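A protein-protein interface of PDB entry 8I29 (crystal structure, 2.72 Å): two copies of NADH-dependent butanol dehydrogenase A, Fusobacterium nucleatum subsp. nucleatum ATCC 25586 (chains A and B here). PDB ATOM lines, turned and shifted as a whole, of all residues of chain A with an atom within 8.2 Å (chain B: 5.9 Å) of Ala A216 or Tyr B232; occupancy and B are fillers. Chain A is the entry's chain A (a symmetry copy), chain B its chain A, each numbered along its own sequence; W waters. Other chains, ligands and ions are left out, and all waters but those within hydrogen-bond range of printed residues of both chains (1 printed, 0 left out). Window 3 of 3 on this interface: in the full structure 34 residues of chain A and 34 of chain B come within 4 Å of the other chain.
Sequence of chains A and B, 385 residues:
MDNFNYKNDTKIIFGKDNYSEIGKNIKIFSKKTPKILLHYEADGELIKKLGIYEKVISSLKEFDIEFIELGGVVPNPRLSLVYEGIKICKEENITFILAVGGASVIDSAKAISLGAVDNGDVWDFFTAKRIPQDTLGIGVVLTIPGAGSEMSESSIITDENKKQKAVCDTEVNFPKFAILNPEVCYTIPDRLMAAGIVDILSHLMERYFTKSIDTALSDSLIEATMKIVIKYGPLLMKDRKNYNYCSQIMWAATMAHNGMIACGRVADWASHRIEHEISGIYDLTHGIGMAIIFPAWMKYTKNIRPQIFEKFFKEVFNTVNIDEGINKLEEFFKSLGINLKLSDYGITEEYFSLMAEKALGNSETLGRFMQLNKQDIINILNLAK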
ATOM      1  N   TYR A 208      29.143 -17.668  30.341  1.00  0.00           N
ATOM      2  CA  TYR A 208      28.517 -17.480  29.047  1.00  0.00           C
ATOM      3  C   TYR A 208      27.031 -17.823  29.128  1.00  0.00           C
ATOM      4  O   TYR A 208      26.193 -16.999  28.762  1.00  0.00           O
ATOM      5  CB  TYR A 208      29.197 -18.332  27.972  1.00  0.00           C
ATOM      6  CG  TYR A 208      28.658 -18.087  26.585  1.00  0.00           C
ATOM      7  CD1 TYR A 208      29.063 -17.020  25.825  1.00  0.00           C
ATOM      8  CD2 TYR A 208      27.681 -18.885  26.051  1.00  0.00           C
ATOM      9  CE1 TYR A 208      28.577 -16.805  24.549  1.00  0.00           C
ATOM     10  CE2 TYR A 208      27.166 -18.670  24.788  1.00  0.00           C
ATOM     11  CZ  TYR A 208      27.618 -17.627  24.020  1.00  0.00           C
ATOM     12  OH  TYR A 208      27.117 -17.450  22.736  1.00  0.00           O
ATOM     13  N   SER A 212      20.794 -13.409  31.267  1.00  0.00           N
ATOM     14  CA  SER A 212      20.999 -11.983  31.026  1.00  0.00           C
ATOM     15  C   SER A 212      20.859 -11.656  29.537  1.00  0.00           C
ATOM     16  O   SER A 212      21.167 -12.490  28.691  1.00  0.00           O
ATOM     17  CB  SER A 212      22.350 -11.527  31.549  1.00  0.00           C
ATOM     18  OG  SER A 212      22.575 -11.951  32.886  1.00  0.00           O
ATOM     19  N   ILE A 213      20.407 -10.435  29.217  1.00  0.00           N
ATOM     20  CA  ILE A 213      20.177 -10.014  27.835  1.00  0.00           C
ATOM     21  C   ILE A 213      21.069  -8.810  27.519  1.00  0.00           C
ATOM     22  O   ILE A 213      21.581  -8.167  28.433  1.00  0.00           O
ATOM     23  CB  ILE A 213      18.676  -9.731  27.545  1.00  0.00           C
ATOM     24  CG1 ILE A 213      17.985  -8.795  28.552  1.00  0.00           C
ATOM     25  CG2 ILE A 213      17.897 -11.028  27.445  1.00  0.00           C
ATOM     26  CD1 ILE A 213      18.409  -7.334  28.503  1.00  0.00           C
ATOM     27  N   ASP A 214      21.247  -8.526  26.218  1.00  0.00           N
ATOM     28  CA  ASP A 214      21.920  -7.336  25.707  1.00  0.00           C
ATOM     29  C   ASP A 214      23.434  -7.426  25.921  1.00  0.00           C
ATOM     30  O   ASP A 214      24.069  -6.428  26.259  1.00  0.00           O
ATOM     31  CB  ASP A 214      21.344  -6.042  26.305  1.00  0.00           C
ATOM     32  CG  ASP A 214      19.990  -5.617  25.736  1.00  0.00           C
ATOM     33  OD1 ASP A 214      19.475  -6.336  24.829  1.00  0.00           O
ATOM     34  OD2 ASP A 214      19.455  -4.550  26.195  1.00  0.00           O
ATOM     35  N   THR A 215      24.026  -8.601  25.666  1.00  0.00           N
ATOM     36  CA  THR A 215      25.410  -8.874  26.046  1.00  0.00           C
ATOM     37  C   THR A 215      26.292  -9.234  24.840  1.00  0.00           C
ATOM     38  O   THR A 215      27.251  -9.984  24.995  1.00  0.00           O
ATOM     39  CB  THR A 215      25.417  -9.980  27.105  1.00  0.00           C
ATOM     40  OG1 THR A 215      24.591 -11.057  26.664  1.00  0.00           O
ATOM     41  CG2 THR A 215      24.893  -9.495  28.430  1.00  0.00           C
ATOM     42  N   ALA A 216      25.989  -8.638  23.671  1.00  0.00           N
ATOM     43  CA  ALA A 216      26.527  -9.022  22.369  1.00  0.00           C
ATOM     44  C   ALA A 216      28.054  -9.004  22.354  1.00  0.00           C
ATOM     45  O   ALA A 216      28.664 -10.037  22.106  1.00  0.00           O
ATOM     46  CB  ALA A 216      25.984  -8.115  21.285  1.00  0.00           C
ATOM     47  N   LEU A 217      28.651  -7.835  22.621  1.00  0.00           N
ATOM     48  CA  LEU A 217      30.099  -7.722  22.639  1.00  0.00           C
ATOM     49  C   LEU A 217      30.716  -8.698  23.641  1.00  0.00           C
ATOM     50  O   LEU A 217      31.672  -9.429  23.323  1.00  0.00           O
ATOM     51  CB  LEU A 217      30.475  -6.279  22.973  1.00  0.00           C
ATOM     52  CG  LEU A 217      31.942  -6.051  23.294  1.00  0.00           C
ATOM     53  CD1 LEU A 217      32.800  -6.574  22.169  1.00  0.00           C
ATOM     54  CD2 LEU A 217      32.193  -4.576  23.514  1.00  0.00           C
ATOM     55  N   SER A 218      30.164  -8.700  24.857  1.00  0.00           N
ATOM     56  CA  SER A 218      30.595  -9.652  25.866  1.00  0.00           C
ATOM     57  C   SER A 218      30.535 -11.085  25.318  1.00  0.00           C
ATOM     58  O   SER A 218      31.479 -11.878  25.449  1.00  0.00           O
ATOM     59  CB  SER A 218      29.766  -9.478  27.085  1.00  0.00           C
ATOM     60  OG  SER A 218      30.134 -10.409  28.079  1.00  0.00           O
ATOM     61  N   ASP A 219      29.425 -11.420  24.662  1.00  0.00           N
ATOM     62  CA  ASP A 219      29.290 -12.740  24.076  1.00  0.00           C
ATOM     63  C   ASP A 219      30.504 -13.009  23.175  1.00  0.00           C
ATOM     64  O   ASP A 219      31.207 -14.008  23.356  1.00  0.00           O
ATOM     65  CB  ASP A 219      27.926 -12.875  23.376  1.00  0.00           C
ATOM     66  CG  ASP A 219      26.699 -13.054  24.272  1.00  0.00           C
ATOM     67  OD1 ASP A 219      26.847 -13.307  25.497  1.00  0.00           O
ATOM     68  OD2 ASP A 219      25.591 -12.972  23.725  1.00  0.00           O
ATOM     69  N   SER A 220      30.759 -12.087  22.234  1.00  0.00           N
ATOM     70  CA  SER A 220      31.824 -12.212  21.247  1.00  0.00           C
ATOM     71  C   SER A 220      33.178 -12.498  21.897  1.00  0.00           C
ATOM     72  O   SER A 220      33.939 -13.339  21.435  1.00  0.00           O
ATOM     73  CB  SER A 220      31.911 -10.956  20.412  1.00  0.00           C
ATOM     74  OG  SER A 220      30.901 -10.937  19.426  1.00  0.00           O
ATOM     75  N   LEU A 221      33.492 -11.744  22.944  1.00  0.00           N
ATOM     76  CA  LEU A 221      34.790 -11.846  23.572  1.00  0.00           C
ATOM     77  C   LEU A 221      34.909 -13.219  24.210  1.00  0.00           C
ATOM     78  O   LEU A 221      35.907 -13.873  23.963  1.00  0.00           O
ATOM     79  CB  LEU A 221      34.968 -10.697  24.562  1.00  0.00           C
ATOM     80  CG  LEU A 221      35.010  -9.304  23.905  1.00  0.00           C
ATOM     81  CD1 LEU A 221      34.660  -8.180  24.869  1.00  0.00           C
ATOM     82  CD2 LEU A 221      36.364  -9.005  23.281  1.00  0.00           C
ATOM     83  N   ILE A 222      33.865 -13.685  24.931  1.00  0.00           N
ATOM     84  CA  ILE A 222      33.896 -14.966  25.637  1.00  0.00           C
ATOM     85  C   ILE A 222      33.948 -16.103  24.631  1.00  0.00           C
ATOM     86  O   ILE A 222      34.599 -17.124  24.886  1.00  0.00           O
ATOM     87  CB  ILE A 222      32.706 -15.139  26.601  1.00  0.00           C
ATOM     88  CG1 ILE A 222      32.756 -14.064  27.696  1.00  0.00           C
ATOM     89  CG2 ILE A 222      32.662 -16.568  27.171  1.00  0.00           C
ATOM     90  CD1 ILE A 222      31.538 -14.021  28.577  1.00  0.00           C
ATOM     91  N   GLU A 223      33.261 -15.903  23.500  1.00  0.00           N
ATOM     92  CA  GLU A 223      33.293 -16.855  22.401  1.00  0.00           C
ATOM     93  C   GLU A 223      34.714 -16.938  21.854  1.00  0.00           C
ATOM     94  O   GLU A 223      35.194 -18.020  21.522  1.00  0.00           O
ATOM     95  CB  GLU A 223      32.341 -16.441  21.282  1.00  0.00           C
ATOM     96  CG  GLU A 223      30.883 -16.525  21.650  1.00  0.00           C
ATOM     97  CD  GLU A 223      29.923 -15.747  20.751  1.00  0.00           C
ATOM     98  OE1 GLU A 223      30.342 -15.183  19.733  1.00  0.00           O
ATOM     99  OE2 GLU A 223      28.738 -15.710  21.072  1.00  0.00           O
ATOM    100  N   ILE A 261      35.510  -9.014  29.910  1.00  0.00           N
ATOM    101  CA  ILE A 261      34.850  -9.768  28.872  1.00  0.00           C
ATOM    102  C   ILE A 261      33.513 -10.243  29.407  1.00  0.00           C
ATOM    103  O   ILE A 261      32.537 -10.113  28.695  1.00  0.00           O
ATOM    104  CB  ILE A 261      35.736 -10.861  28.250  1.00  0.00           C
ATOM    105  CG1 ILE A 261      36.223 -11.893  29.270  1.00  0.00           C
ATOM    106  CG2 ILE A 261      36.889 -10.218  27.484  1.00  0.00           C
ATOM    107  CD1 ILE A 261      36.380 -13.294  28.699  1.00  0.00           C
ATOM    108  N   ARG A 265      27.119  -9.752  33.459  1.00  0.00           N
ATOM    109  CA  ARG A 265      26.292 -10.898  33.112  1.00  0.00           C
ATOM    110  C   ARG A 265      26.346 -11.934  34.243  1.00  0.00           C
ATOM    111  O   ARG A 265      27.350 -12.016  34.964  1.00  0.00           O
ATOM    112  CB  ARG A 265      26.796 -11.515  31.806  1.00  0.00           C
ATOM    113  CG  ARG A 265      28.161 -12.168  31.947  1.00  0.00           C
ATOM    114  CD  ARG A 265      28.755 -12.492  30.601  1.00  0.00           C
ATOM    115  NE  ARG A 265      27.974 -13.503  29.922  1.00  0.00           N
ATOM    116  CZ  ARG A 265      27.635 -13.457  28.647  1.00  0.00           C
ATOM    117  NH1 ARG A 265      26.992 -14.467  28.096  1.00  0.00           N
ATOM    118  NH2 ARG A 265      27.975 -12.422  27.905  1.00  0.00           N
ATOM    119  N   LYS A 311      23.550 -20.225  19.637  1.00  0.00           N
ATOM    120  CA  LYS A 311      24.636 -19.281  19.433  1.00  0.00           C
ATOM    121  C   LYS A 311      25.974 -19.903  19.854  1.00  0.00           C
ATOM    122  O   LYS A 311      26.913 -19.954  19.070  1.00  0.00           O
ATOM    123  CB  LYS A 311      24.382 -17.986  20.192  1.00  0.00           C
ATOM    124  CG  LYS A 311      25.320 -16.857  19.789  1.00  0.00           C
ATOM    125  CD  LYS A 311      24.965 -15.545  20.445  1.00  0.00           C
ATOM    126  CE  LYS A 311      25.801 -14.374  19.983  1.00  0.00           C
ATOM    127  NZ  LYS A 311      25.520 -13.199  20.837  1.00  0.00           N
ATOM    128  N   LYS B 227      33.974  -6.565  14.765  1.00  0.00           N
ATOM    129  CA  LYS B 227      32.730  -7.100  14.227  1.00  0.00           C
ATOM    130  C   LYS B 227      31.515  -6.424  14.850  1.00  0.00           C
ATOM    131  O   LYS B 227      30.522  -6.169  14.165  1.00  0.00           O
ATOM    132  CB  LYS B 227      32.554  -8.582  14.549  1.00  0.00           C
ATOM    133  CG  LYS B 227      33.390  -9.545  13.732  1.00  0.00           C
ATOM    134  CD  LYS B 227      32.818 -10.945  13.707  1.00  0.00           C
ATOM    135  CE  LYS B 227      31.643 -11.062  12.751  1.00  0.00           C
ATOM    136  NZ  LYS B 227      31.227 -12.473  12.560  1.00  0.00           N
ATOM    137  N   ILE B 228      31.600  -6.208  16.168  1.00  0.00           N
ATOM    138  CA  ILE B 228      30.528  -5.589  16.925  1.00  0.00           C
ATOM    139  C   ILE B 228      30.414  -4.150  16.459  1.00  0.00           C
ATOM    140  O   ILE B 228      29.308  -3.669  16.223  1.00  0.00           O
ATOM    141  CB  ILE B 228      30.774  -5.705  18.447  1.00  0.00           C
ATOM    142  CG1 ILE B 228      30.451  -7.101  18.981  1.00  0.00           C
ATOM    143  CG2 ILE B 228      30.012  -4.664  19.226  1.00  0.00           C
ATOM    144  CD1 ILE B 228      28.992  -7.431  18.992  1.00  0.00           C
ATOM    145  N   VAL B 229      31.554  -3.478  16.288  1.00  0.00           N
ATOM    146  CA  VAL B 229      31.482  -2.135  15.756  1.00  0.00           C
ATOM    147  C   VAL B 229      30.803  -2.220  14.388  1.00  0.00           C
ATOM    148  O   VAL B 229      29.923  -1.416  14.075  1.00  0.00           O
ATOM    149  CB  VAL B 229      32.869  -1.463  15.765  1.00  0.00           C
ATOM    150  CG1 VAL B 229      32.895  -0.112  15.069  1.00  0.00           C
ATOM    151  CG2 VAL B 229      33.361  -1.293  17.195  1.00  0.00           C
ATOM    152  N   ILE B 230      31.136  -3.229  13.582  1.00  0.00           N
ATOM    153  CA  ILE B 230      30.623  -3.261  12.214  1.00  0.00           C
ATOM    154  C   ILE B 230      29.109  -3.552  12.230  1.00  0.00           C
ATOM    155  O   ILE B 230      28.351  -3.095  11.345  1.00  0.00           O
ATOM    156  CB  ILE B 230      31.441  -4.274  11.370  1.00  0.00           C
ATOM    157  CG1 ILE B 230      32.931  -3.903  11.272  1.00  0.00           C
ATOM    158  CG2 ILE B 230      30.850  -4.472   9.987  1.00  0.00           C
ATOM    159  CD1 ILE B 230      33.209  -2.633  10.573  1.00  0.00           C
ATOM    160  N   LYS B 231      28.672  -4.339  13.230  1.00  0.00           N
ATOM    161  CA  LYS B 231      27.298  -4.797  13.287  1.00  0.00           C
ATOM    162  C   LYS B 231      26.406  -3.734  13.950  1.00  0.00           C
ATOM    163  O   LYS B 231      25.402  -3.347  13.383  1.00  0.00           O
ATOM    164  CB  LYS B 231      27.279  -6.154  13.986  1.00  0.00           C
ATOM    165  CG  LYS B 231      25.927  -6.849  14.004  1.00  0.00           C
ATOM    166  CD  LYS B 231      25.938  -8.179  14.701  1.00  0.00           C
ATOM    167  CE  LYS B 231      24.560  -8.704  15.063  1.00  0.00           C
ATOM    168  NZ  LYS B 231      24.569  -9.417  16.377  1.00  0.00           N
ATOM    169  N   TYR B 232      26.795  -3.197  15.108  1.00  0.00           N
ATOM    170  CA  TYR B 232      25.928  -2.302  15.861  1.00  0.00           C
ATOM    171  C   TYR B 232      25.989  -0.844  15.387  1.00  0.00           C
ATOM    172  O   TYR B 232      24.957  -0.164  15.376  1.00  0.00           O
ATOM    173  CB  TYR B 232      26.179  -2.487  17.368  1.00  0.00           C
ATOM    174  CG  TYR B 232      25.514  -3.746  17.882  1.00  0.00           C
ATOM    175  CD1 TYR B 232      26.121  -4.987  17.736  1.00  0.00           C
ATOM    176  CD2 TYR B 232      24.228  -3.726  18.395  1.00  0.00           C
ATOM    177  CE1 TYR B 232      25.498  -6.156  18.131  1.00  0.00           C
ATOM    178  CE2 TYR B 232      23.589  -4.890  18.796  1.00  0.00           C
ATOM    179  CZ  TYR B 232      24.212  -6.117  18.645  1.00  0.00           C
ATOM    180  OH  TYR B 232      23.560  -7.280  19.023  1.00  0.00           O
ATOM    181  N   GLY B 233      27.175  -0.360  14.994  1.00  0.00           N
ATOM    182  CA  GLY B 233      27.391   1.041  14.648  1.00  0.00           C
ATOM    183  C   GLY B 233      26.375   1.546  13.626  1.00  0.00           C
ATOM    184  O   GLY B 233      25.807   2.604  13.786  1.00  0.00           O
ATOM    185  N   PRO B 234      26.074   0.778  12.569  1.00  0.00           N
ATOM    186  CA  PRO B 234      24.982   1.109  11.650  1.00  0.00           C
ATOM    187  C   PRO B 234      23.581   1.120  12.276  1.00  0.00           C
ATOM    188  O   PRO B 234      22.705   1.901  11.882  1.00  0.00           O
ATOM    189  CB  PRO B 234      25.023  -0.042  10.616  1.00  0.00           C
ATOM    190  CG  PRO B 234      26.399  -0.684  10.774  1.00  0.00           C
ATOM    191  CD  PRO B 234      26.736  -0.495  12.238  1.00  0.00           C
ATOM    192  N   LEU B 235      23.344   0.210  13.234  1.00  0.00           N
ATOM    193  CA  LEU B 235      22.066   0.172  13.916  1.00  0.00           C
ATOM    194  C   LEU B 235      21.936   1.401  14.826  1.00  0.00           C
ATOM    195  O   LEU B 235      20.911   2.086  14.852  1.00  0.00           O
ATOM    196  CB  LEU B 235      21.971  -1.144  14.687  1.00  0.00           C
ATOM    197  CG  LEU B 235      22.310  -2.424  13.917  1.00  0.00           C
ATOM    198  CD1 LEU B 235      22.236  -3.628  14.845  1.00  0.00           C
ATOM    199  CD2 LEU B 235      21.387  -2.647  12.749  1.00  0.00           C
ATOM    200  N   LEU B 236      23.005   1.727  15.554  1.00  0.00           N
ATOM    201  CA  LEU B 236      22.996   2.903  16.416  1.00  0.00           C
ATOM    202  C   LEU B 236      22.700   4.152  15.590  1.00  0.00           C
ATOM    203  O   LEU B 236      22.007   5.042  16.046  1.00  0.00           O
ATOM    204  CB  LEU B 236      24.349   2.985  17.131  1.00  0.00           C
ATOM    205  CG  LEU B 236      24.527   4.042  18.219  1.00  0.00           C
ATOM    206  CD1 LEU B 236      25.731   3.724  19.095  1.00  0.00           C
ATOM    207  CD2 LEU B 236      24.734   5.411  17.616  1.00  0.00           C
ATOM    208  N   MET B 237      23.220   4.219  14.363  1.00  0.00           N
ATOM    209  CA  MET B 237      23.063   5.421  13.566  1.00  0.00           C
ATOM    210  C   MET B 237      21.592   5.618  13.226  1.00  0.00           C
ATOM    211  O   MET B 237      21.147   6.750  13.145  1.00  0.00           O
ATOM    212  CB  MET B 237      23.900   5.372  12.289  1.00  0.00           C
ATOM    213  CG  MET B 237      25.359   5.658  12.569  1.00  0.00           C
ATOM    214  SD  MET B 237      25.757   7.259  13.349  1.00  0.00           S
ATOM    215  CE  MET B 237      25.134   8.339  12.064  1.00  0.00           C
ATOM    216  N   ASN B 244      20.850  -0.501  24.235  1.00  0.00           N
ATOM    217  CA  ASN B 244      21.617  -1.678  23.857  1.00  0.00           C
ATOM    218  C   ASN B 244      22.677  -1.300  22.828  1.00  0.00           C
ATOM    219  O   ASN B 244      23.854  -1.556  23.055  1.00  0.00           O
ATOM    220  CB  ASN B 244      20.692  -2.798  23.362  1.00  0.00           C
ATOM    221  CG  ASN B 244      21.397  -4.032  22.836  1.00  0.00           C
ATOM    222  OD1 ASN B 244      22.405  -4.507  23.365  1.00  0.00           O
ATOM    223  ND2 ASN B 244      20.852  -4.577  21.774  1.00  0.00           N
ATOM    224  N   TYR B 245      22.247  -0.716  21.707  1.00  0.00           N
ATOM    225  CA  TYR B 245      23.152  -0.364  20.622  1.00  0.00           C
ATOM    226  C   TYR B 245      24.271   0.549  21.134  1.00  0.00           C
ATOM    227  O   TYR B 245      25.441   0.357  20.786  1.00  0.00           O
ATOM    228  CB  TYR B 245      22.394   0.310  19.476  1.00  0.00           C
ATOM    229  CG  TYR B 245      21.334  -0.533  18.804  1.00  0.00           C
ATOM    230  CD1 TYR B 245      21.159  -1.880  19.097  1.00  0.00           C
ATOM    231  CD2 TYR B 245      20.490   0.030  17.854  1.00  0.00           C
ATOM    232  CE1 TYR B 245      20.207  -2.647  18.446  1.00  0.00           C
ATOM    233  CE2 TYR B 245      19.520  -0.713  17.208  1.00  0.00           C
ATOM    234  CZ  TYR B 245      19.384  -2.057  17.502  1.00  0.00           C
ATOM    235  OH  TYR B 245      18.417  -2.786  16.869  1.00  0.00           O
ATOM    236  N   GLN B 248      26.733  -1.544  23.488  1.00  0.00           N
ATOM    237  CA  GLN B 248      27.737  -2.317  22.784  1.00  0.00           C
ATOM    238  C   GLN B 248      28.847  -1.365  22.303  1.00  0.00           C
ATOM    239  O   GLN B 248      30.031  -1.552  22.596  1.00  0.00           O
ATOM    240  CB  GLN B 248      27.065  -3.125  21.671  1.00  0.00           C
ATOM    241  CG  GLN B 248      25.911  -4.001  22.144  1.00  0.00           C
ATOM    242  CD  GLN B 248      26.307  -4.772  23.367  1.00  0.00           C
ATOM    243  OE1 GLN B 248      27.309  -5.491  23.401  1.00  0.00           O
ATOM    244  NE2 GLN B 248      25.547  -4.553  24.415  1.00  0.00           N
ATOM    245  N   ILE B 249      28.452  -0.283  21.632  1.00  0.00           N
ATOM    246  CA  ILE B 249      29.393   0.630  21.020  1.00  0.00           C
ATOM    247  C   ILE B 249      30.288   1.308  22.060  1.00  0.00           C
ATOM    248  O   ILE B 249      31.511   1.367  21.918  1.00  0.00           O
ATOM    249  CB  ILE B 249      28.617   1.612  20.138  1.00  0.00           C
ATOM    250  CG1 ILE B 249      27.988   0.854  18.986  1.00  0.00           C
ATOM    251  CG2 ILE B 249      29.519   2.713  19.620  1.00  0.00           C
ATOM    252  CD1 ILE B 249      29.032   0.191  18.100  1.00  0.00           C
HETATM  253  O   HOH W   1      23.178  -6.993  22.731  1.00  0.00           O
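The backbone NH (N) of Leu A217 is in hydrogen-bond range of the side-chain amide oxygen (OE1) of Gln B248 (2.8 Å). O of Asp A214 lies within hydrogen-bond range of NE2 of Gln B248 (3.0 Å). OE1 of Gln B248 lies within hydrogen-bond range of N of Ala A216 (3.4 Å).
The side-chain amide oxygen (OD1) of Asn B244 lies within hydrogen-bond range of the side-chain amide nitrogen (NE2) of Gln B248 (3.3 Å).
Among the printed residues, pairs that only touch across the chains: Ala A216 with Tyr B232 (3.4 Å), Asp A214 with Asn B244 (3.5 Å), Leu A217 with Ile B228 (3.7 Å), Ala A216 with Ile B228 (3.8 Å) and Ser A220 with Ile B228 (3.9 Å).
Ala A216 touches three residues of chain B. No residue of chain A comes within 4 Å of Lys B231. No residue of chain A comes within 4 Å of Gly B233. Printed residues of chain B within 4 Å of Leu A217: Ile B228 and Gln B248. Of the printed residues of chain B, Asp A214 touches Asn B244 (3.5 Å) and Gln B248 (3.0 Å). Of the printed residues of chain A, Ile B228 touches Ala A216, Leu A217 and Ser A220. Of the printed residues of chain A, Gln B248 touches Asp A214 (3.0 Å), Ala A216 (3.4 Å) and Leu A217 (2.8 Å). Of the printed residues of chain B, Ser A220 touches Ile B228 (3.9 Å). Ser A218 touches none of the printed residues of chain B. Glu A223 touches none of the printed residues of chain B.
Of the 16 printed residues of chain A, 4 touch a printed residue of chain B. Hydrophobic or aromatic side chains of chain A that line the printed part of chain B: Ala A216 and Leu A217. Of the 15 printed residues of chain B, 4 touch a printed residue of chain A. Printed residues of chain B that touch a printed residue of chain A: Ile B228, Tyr B232, Asn B244 and Gln B248. Hydrophobic or aromatic side chains of chain B that line the printed part of chain A: Ile B228 and Tyr B232. Among the printed residues, no Asp or Glu carboxylate lies within 4 Å of a Lys or Arg side-chain nitrogen of the other chain.
No position is printed for both chains.
Water W1 lies within hydrogen-bond range of OD1 of Asn B244 (2.7 Å), N of Ala A216 (3.4 Å) and N of Thr A215 (3.5 Å).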
